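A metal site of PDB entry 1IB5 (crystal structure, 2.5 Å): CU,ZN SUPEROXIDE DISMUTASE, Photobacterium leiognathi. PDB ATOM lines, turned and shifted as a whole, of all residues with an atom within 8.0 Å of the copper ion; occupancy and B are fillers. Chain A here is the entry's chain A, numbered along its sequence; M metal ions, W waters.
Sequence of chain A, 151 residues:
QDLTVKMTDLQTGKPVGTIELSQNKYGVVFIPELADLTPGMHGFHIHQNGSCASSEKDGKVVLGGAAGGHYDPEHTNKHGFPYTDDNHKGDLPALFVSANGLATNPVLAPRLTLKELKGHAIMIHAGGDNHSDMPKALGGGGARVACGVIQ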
ATOM      1  N   GLY A  43      -0.294 -23.643 -13.256  1.00  0.00           N
ATOM      2  CA  GLY A  43      -0.487 -24.395 -12.034  1.00  0.00           C
ATOM      3  C   GLY A  43      -1.881 -24.066 -11.535  1.00  0.00           C
ATOM      4  O   GLY A  43      -2.249 -22.898 -11.457  1.00  0.00           O
ATOM      5  N   PHE A  44      -2.646 -25.094 -11.202  1.00  0.00           N
ATOM      6  CA  PHE A  44      -4.023 -24.929 -10.763  1.00  0.00           C
ATOM      7  C   PHE A  44      -4.237 -25.698  -9.474  1.00  0.00           C
ATOM      8  O   PHE A  44      -4.190 -26.926  -9.461  1.00  0.00           O
ATOM      9  CB  PHE A  44      -4.910 -25.456 -11.887  1.00  0.00           C
ATOM     10  CG  PHE A  44      -6.352 -25.108 -11.754  1.00  0.00           C
ATOM     11  CD1 PHE A  44      -6.759 -23.856 -11.293  1.00  0.00           C
ATOM     12  CD2 PHE A  44      -7.314 -26.021 -12.139  1.00  0.00           C
ATOM     13  CE1 PHE A  44      -8.096 -23.505 -11.282  1.00  0.00           C
ATOM     14  CE2 PHE A  44      -8.643 -25.674 -12.126  1.00  0.00           C
ATOM     15  CZ  PHE A  44      -9.037 -24.426 -11.678  1.00  0.00           C
ATOM     16  N   HIS A  45      -4.455 -24.981  -8.379  1.00  0.00           N
ATOM     17  CA  HIS A  45      -4.610 -25.659  -7.092  1.00  0.00           C
ATOM     18  C   HIS A  45      -5.662 -25.089  -6.158  1.00  0.00           C
ATOM     19  O   HIS A  45      -6.076 -23.927  -6.279  1.00  0.00           O
ATOM     20  CB  HIS A  45      -3.288 -25.611  -6.328  1.00  0.00           C
ATOM     21  CG  HIS A  45      -2.083 -25.898  -7.170  1.00  0.00           C
ATOM     22  ND1 HIS A  45      -0.990 -25.071  -7.184  1.00  0.00           N
ATOM     23  CD2 HIS A  45      -1.808 -26.921  -8.007  1.00  0.00           C
ATOM     24  CE1 HIS A  45      -0.080 -25.568  -8.006  1.00  0.00           C
ATOM     25  NE2 HIS A  45      -0.557 -26.693  -8.517  1.00  0.00           N
ATOM     26  N   ILE A  46      -6.102 -25.909  -5.213  1.00  0.00           N
ATOM     27  CA  ILE A  46      -7.028 -25.440  -4.193  1.00  0.00           C
ATOM     28  C   ILE A  46      -6.096 -25.160  -3.013  1.00  0.00           C
ATOM     29  O   ILE A  46      -5.242 -25.970  -2.679  1.00  0.00           O
ATOM     30  CB  ILE A  46      -8.038 -26.515  -3.780  1.00  0.00           C
ATOM     31  CG1 ILE A  46      -9.053 -26.781  -4.906  1.00  0.00           C
ATOM     32  CG2 ILE A  46      -8.744 -26.062  -2.516  1.00  0.00           C
ATOM     33  CD1 ILE A  46      -9.894 -25.570  -5.293  1.00  0.00           C
ATOM     34  N   HIS A  47      -6.244 -23.992  -2.392  1.00  0.00           N
ATOM     35  CA  HIS A  47      -5.389 -23.658  -1.260  1.00  0.00           C
ATOM     36  C   HIS A  47      -6.084 -23.750   0.081  1.00  0.00           C
ATOM     37  O   HIS A  47      -7.315 -23.834   0.149  1.00  0.00           O
ATOM     38  CB  HIS A  47      -4.756 -22.282  -1.445  1.00  0.00           C
ATOM     39  CG  HIS A  47      -3.587 -22.278  -2.389  1.00  0.00           C
ATOM     40  ND1 HIS A  47      -2.338 -21.851  -2.021  1.00  0.00           N
ATOM     41  CD2 HIS A  47      -3.486 -22.696  -3.677  1.00  0.00           C
ATOM     42  CE1 HIS A  47      -1.510 -22.002  -3.038  1.00  0.00           C
ATOM     43  NE2 HIS A  47      -2.171 -22.516  -4.053  1.00  0.00           N
ATOM     44  N   GLY A  68      -2.480 -19.250   1.978  1.00  0.00           N
ATOM     45  CA  GLY A  68      -1.683 -20.295   2.579  1.00  0.00           C
ATOM     46  C   GLY A  68      -1.203 -21.283   1.530  1.00  0.00           C
ATOM     47  O   GLY A  68      -1.199 -20.995   0.339  1.00  0.00           O
ATOM     48  N   GLY A  69      -0.779 -22.458   1.994  1.00  0.00           N
ATOM     49  CA  GLY A  69      -0.280 -23.485   1.106  1.00  0.00           C
ATOM     50  C   GLY A  69      -1.395 -24.282   0.456  1.00  0.00           C
ATOM     51  O   GLY A  69      -2.563 -23.882   0.487  1.00  0.00           O
ATOM     52  N   HIS A  70      -1.051 -25.415  -0.141  1.00  0.00           N
ATOM     53  CA  HIS A  70      -2.036 -26.251  -0.801  1.00  0.00           C
ATOM     54  C   HIS A  70      -2.915 -27.001   0.189  1.00  0.00           C
ATOM     55  O   HIS A  70      -2.507 -27.310   1.317  1.00  0.00           O
ATOM     56  CB  HIS A  70      -1.348 -27.240  -1.739  1.00  0.00           C
ATOM     57  CG  HIS A  70      -0.656 -26.582  -2.901  1.00  0.00           C
ATOM     58  ND1 HIS A  70       0.134 -27.289  -3.787  1.00  0.00           N
ATOM     59  CD2 HIS A  70      -0.657 -25.302  -3.321  1.00  0.00           C
ATOM     60  CE1 HIS A  70       0.591 -26.449  -4.712  1.00  0.00           C
ATOM     61  NE2 HIS A  70       0.131 -25.239  -4.448  1.00  0.00           N
ATOM     62  N   TYR A  71      -4.136 -27.281  -0.228  1.00  0.00           N
ATOM     63  CA  TYR A  71      -5.090 -27.995   0.588  1.00  0.00           C
ATOM     64  C   TYR A  71      -4.472 -29.376   0.840  1.00  0.00           C
ATOM     65  O   TYR A  71      -4.208 -30.128  -0.102  1.00  0.00           O
ATOM     66  CB  TYR A  71      -6.413 -28.089  -0.179  1.00  0.00           C
ATOM     67  CG  TYR A  71      -7.544 -28.758   0.549  1.00  0.00           C
ATOM     68  CD1 TYR A  71      -7.866 -28.404   1.863  1.00  0.00           C
ATOM     69  CD2 TYR A  71      -8.302 -29.758  -0.072  1.00  0.00           C
ATOM     70  CE1 TYR A  71      -8.903 -29.021   2.537  1.00  0.00           C
ATOM     71  CE2 TYR A  71      -9.350 -30.394   0.605  1.00  0.00           C
ATOM     72  CZ  TYR A  71      -9.640 -30.029   1.904  1.00  0.00           C
ATOM     73  OH  TYR A  71     -10.656 -30.666   2.589  1.00  0.00           O
ATOM     74  N   HIS A  79       3.697 -32.446  -2.884  1.00  0.00           N
ATOM     75  CA  HIS A  79       2.916 -31.979  -4.019  1.00  0.00           C
ATOM     76  C   HIS A  79       2.967 -33.123  -5.038  1.00  0.00           C
ATOM     77  O   HIS A  79       3.994 -33.782  -5.156  1.00  0.00           O
ATOM     78  CB  HIS A  79       3.506 -30.699  -4.612  1.00  0.00           C
ATOM     79  CG  HIS A  79       2.805 -30.221  -5.844  1.00  0.00           C
ATOM     80  ND1 HIS A  79       1.511 -29.717  -5.827  1.00  0.00           N
ATOM     81  CD2 HIS A  79       3.187 -30.214  -7.153  1.00  0.00           C
ATOM     82  CE1 HIS A  79       1.152 -29.419  -7.068  1.00  0.00           C
ATOM     83  NE2 HIS A  79       2.134 -29.707  -7.880  1.00  0.00           N
ATOM     84  N   HIS A  88      -0.972 -33.565  -1.504  1.00  0.00           N
ATOM     85  CA  HIS A  88      -1.980 -32.530  -1.361  1.00  0.00           C
ATOM     86  C   HIS A  88      -3.279 -32.933  -2.073  1.00  0.00           C
ATOM     87  O   HIS A  88      -3.273 -33.129  -3.278  1.00  0.00           O
ATOM     88  CB  HIS A  88      -1.465 -31.220  -1.961  1.00  0.00           C
ATOM     89  CG  HIS A  88      -0.182 -30.757  -1.364  1.00  0.00           C
ATOM     90  ND1 HIS A  88       0.796 -30.096  -2.084  1.00  0.00           N
ATOM     91  CD2 HIS A  88       0.295 -30.862  -0.096  1.00  0.00           C
ATOM     92  CE1 HIS A  88       1.812 -29.811  -1.284  1.00  0.00           C
ATOM     93  NE2 HIS A  88       1.534 -30.271  -0.080  1.00  0.00           N
ATOM     94  N   GLY A  90      -5.379 -31.126  -2.690  1.00  0.00           N
ATOM     95  CA  GLY A  90      -5.692 -29.949  -3.500  1.00  0.00           C
ATOM     96  C   GLY A  90      -4.921 -29.823  -4.793  1.00  0.00           C
ATOM     97  O   GLY A  90      -4.943 -28.772  -5.431  1.00  0.00           O
ATOM     98  N   ASP A  91      -4.235 -30.887  -5.192  1.00  0.00           N
ATOM     99  CA  ASP A  91      -3.483 -30.890  -6.426  1.00  0.00           C
ATOM    100  C   ASP A  91      -4.415 -31.211  -7.602  1.00  0.00           C
ATOM    101  O   ASP A  91      -4.827 -32.343  -7.808  1.00  0.00           O
ATOM    102  CB  ASP A  91      -2.349 -31.898  -6.314  1.00  0.00           C
ATOM    103  CG  ASP A  91      -1.356 -31.517  -5.243  1.00  0.00           C
ATOM    104  OD1 ASP A  91      -1.212 -30.299  -5.010  1.00  0.00           O
ATOM    105  OD2 ASP A  91      -0.702 -32.403  -4.655  1.00  0.00           O
ATOM    106  N   ALA A 121      -9.829 -21.540  -1.250  1.00  0.00           N
ATOM    107  CA  ALA A 121      -9.633 -20.668  -2.398  1.00  0.00           C
ATOM    108  C   ALA A 121      -8.971 -21.371  -3.574  1.00  0.00           C
ATOM    109  O   ALA A 121      -8.047 -22.169  -3.398  1.00  0.00           O
ATOM    110  CB  ALA A 121      -8.823 -19.446  -1.994  1.00  0.00           C
ATOM    111  N   ILE A 122      -9.452 -21.076  -4.778  1.00  0.00           N
ATOM    112  CA  ILE A 122      -8.899 -21.655  -5.998  1.00  0.00           C
ATOM    113  C   ILE A 122      -7.760 -20.718  -6.386  1.00  0.00           C
ATOM    114  O   ILE A 122      -7.918 -19.505  -6.330  1.00  0.00           O
ATOM    115  CB  ILE A 122      -9.905 -21.690  -7.141  1.00  0.00           C
ATOM    116  CG1 ILE A 122     -11.138 -22.485  -6.713  1.00  0.00           C
ATOM    117  CG2 ILE A 122      -9.260 -22.336  -8.367  1.00  0.00           C
ATOM    118  CD1 ILE A 122     -12.251 -22.471  -7.759  1.00  0.00           C
ATOM    119  N   MET A 123      -6.642 -21.281  -6.789  1.00  0.00           N
ATOM    120  CA  MET A 123      -5.498 -20.456  -7.147  1.00  0.00           C
ATOM    121  C   MET A 123      -4.943 -20.782  -8.537  1.00  0.00           C
ATOM    122  O   MET A 123      -4.946 -21.929  -8.958  1.00  0.00           O
ATOM    123  CB  MET A 123      -4.397 -20.624  -6.100  1.00  0.00           C
ATOM    124  CG  MET A 123      -3.284 -19.600  -6.160  1.00  0.00           C
ATOM    125  SD  MET A 123      -3.837 -18.010  -5.503  1.00  0.00           S
ATOM    126  CE  MET A 123      -4.050 -18.394  -3.756  1.00  0.00           C
ATOM    127  N   ILE A 124      -4.480 -19.758  -9.221  1.00  0.00           N
ATOM    128  CA  ILE A 124      -3.883 -19.933 -10.539  1.00  0.00           C
ATOM    129  C   ILE A 124      -2.508 -19.293 -10.497  1.00  0.00           C
ATOM    130  O   ILE A 124      -2.362 -18.120 -10.158  1.00  0.00           O
ATOM    131  CB  ILE A 124      -4.719 -19.277 -11.650  1.00  0.00           C
ATOM    132  CG1 ILE A 124      -6.038 -20.032 -11.819  1.00  0.00           C
ATOM    133  CG2 ILE A 124      -3.924 -19.264 -12.954  1.00  0.00           C
ATOM    134  CD1 ILE A 124      -6.923 -19.466 -12.919  1.00  0.00           C
ATOM    135  N   HIS A 125      -1.489 -20.072 -10.851  1.00  0.00           N
ATOM    136  CA  HIS A 125      -0.123 -19.595 -10.852  1.00  0.00           C
ATOM    137  C   HIS A 125       0.353 -19.167 -12.232  1.00  0.00           C
ATOM    138  O   HIS A 125      -0.356 -19.326 -13.230  1.00  0.00           O
ATOM    139  CB  HIS A 125       0.797 -20.679 -10.284  1.00  0.00           C
ATOM    140  CG  HIS A 125       0.485 -21.041  -8.870  1.00  0.00           C
ATOM    141  ND1 HIS A 125       1.428 -20.999  -7.858  1.00  0.00           N
ATOM    142  CD2 HIS A 125      -0.663 -21.461  -8.279  1.00  0.00           C
ATOM    143  CE1 HIS A 125       0.876 -21.371  -6.715  1.00  0.00           C
ATOM    144  NE2 HIS A 125      -0.392 -21.653  -6.947  1.00  0.00           N
ATOM    145  N   ASP A 129       3.039 -26.805 -13.854  1.00  0.00           N
ATOM    146  CA  ASP A 129       2.978 -27.737 -12.739  1.00  0.00           C
ATOM    147  C   ASP A 129       3.406 -29.117 -13.248  1.00  0.00           C
ATOM    148  O   ASP A 129       2.724 -29.694 -14.075  1.00  0.00           O
ATOM    149  CB  ASP A 129       1.526 -27.803 -12.232  1.00  0.00           C
ATOM    150  CG  ASP A 129       1.358 -28.680 -10.999  1.00  0.00           C
ATOM    151  OD1 ASP A 129       2.284 -29.422 -10.615  1.00  0.00           O
ATOM    152  OD2 ASP A 129       0.266 -28.612 -10.395  1.00  0.00           O
ATOM    153  N   LEU A 138       6.420 -27.526  -5.431  1.00  0.00           N
ATOM    154  CA  LEU A 138       5.058 -27.232  -5.822  1.00  0.00           C
ATOM    155  C   LEU A 138       4.833 -27.259  -7.342  1.00  0.00           C
ATOM    156  O   LEU A 138       3.959 -26.574  -7.856  1.00  0.00           O
ATOM    157  CB  LEU A 138       4.663 -25.872  -5.242  1.00  0.00           C
ATOM    158  CG  LEU A 138       4.851 -25.804  -3.720  1.00  0.00           C
ATOM    159  CD1 LEU A 138       4.546 -24.400  -3.189  1.00  0.00           C
ATOM    160  CD2 LEU A 138       3.937 -26.828  -3.063  1.00  0.00           C
ATOM    161  N   GLY A 141       5.039 -23.799 -10.124  1.00  0.00           N
ATOM    162  CA  GLY A 141       3.999 -22.849 -10.474  1.00  0.00           C
ATOM    163  C   GLY A 141       4.400 -21.430 -10.147  1.00  0.00           C
ATOM    164  O   GLY A 141       3.825 -20.487 -10.691  1.00  0.00           O
ATOM    165  N   GLY A 142       5.363 -21.280  -9.253  1.00  0.00           N
ATOM    166  CA  GLY A 142       5.826 -19.965  -8.876  1.00  0.00           C
ATOM    167  C   GLY A 142       4.754 -19.057  -8.306  1.00  0.00           C
ATOM    168  O   GLY A 142       3.885 -19.498  -7.553  1.00  0.00           O
ATOM    169  N   ALA A 143       4.821 -17.785  -8.683  1.00  0.00           N
ATOM    170  CA  ALA A 143       3.889 -16.757  -8.225  1.00  0.00           C
ATOM    171  C   ALA A 143       2.418 -17.069  -8.497  1.00  0.00           C
ATOM    172  O   ALA A 143       2.086 -17.870  -9.379  1.00  0.00           O
ATOM    173  CB  ALA A 143       4.256 -15.411  -8.849  1.00  0.00           C
ATOM    174  N   ARG A 144       1.549 -16.411  -7.748  1.00  0.00           N
ATOM    175  CA  ARG A 144       0.102 -16.580  -7.866  1.00  0.00           C
ATOM    176  C   ARG A 144      -0.446 -15.443  -8.753  1.00  0.00           C
ATOM    177  O   ARG A 144      -0.132 -14.287  -8.509  1.00  0.00           O
ATOM    178  CB  ARG A 144      -0.511 -16.516  -6.465  1.00  0.00           C
ATOM    179  CG  ARG A 144       0.357 -17.251  -5.440  1.00  0.00           C
ATOM    180  CD  ARG A 144      -0.256 -17.391  -4.055  1.00  0.00           C
ATOM    181  NE  ARG A 144       0.615 -18.207  -3.210  1.00  0.00           N
ATOM    182  CZ  ARG A 144       0.239 -18.819  -2.090  1.00  0.00           C
ATOM    183  NH1 ARG A 144      -1.006 -18.733  -1.657  1.00  0.00           N
ATOM    184  NH2 ARG A 144       1.120 -19.539  -1.402  1.00  0.00           N
HETATM  185 CU    CU M   1      -1.119 -23.364  -5.770  1.00  0.00          CU
HETATM  186 ZN    ZN M   2       0.210 -29.364  -4.093  1.00  0.00          ZN
HETATM  187  O   HOH W   1       1.592 -23.261  -4.460  1.00  0.00           O
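NE2 of His 47 binds the copper ion.
The copper ion is bound by a ring nitrogen (NE2) of His 125, at 2.2 Å.
ND1 of His 45 binds the copper ion (2.2 Å).
The copper ion has three donor atoms within binding distance.
Slightly farther from the copper ion lies a ring nitrogen (NE2) of His 70 (2.6 Å).
ND1 of His 45 sits close to NE2 of His 70 (3.0 Å).
N of His 47 sits at hydrogen-bond distance from O of Ala 121 (2.8 Å).
A ring nitrogen (ND1) of His 47 sits at hydrogen-bond distance from the backbone carbonyl oxygen (O) of Gly 69 (3.2 Å).
A ring nitrogen (NE2) of His 45 sits at hydrogen-bond distance from the side-chain carboxylate (OD2) of Asp 129 (2.8 Å).
A ring nitrogen (ND1) of His 125 sits at hydrogen-bond distance from the backbone carbonyl oxygen of Gly 142, 2.9 Å away.
ND1 of His 47 lies within hydrogen-bond range of O of Gly 68.
The backbone carbonyl oxygen (O) of His 45 lies within hydrogen-bond range of the backbone NH (N) of Met 123.
The backbone NH (N) of His 125 is in hydrogen-bond range of the backbone carbonyl oxygen (O) of Gly 43 (3.0 Å).
Within 4 Å of the copper ion: His 45, His 47, His 70 and His 125.
The nearest printed residue that does not touch the copper ion is Met 123 (4.3 Å).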
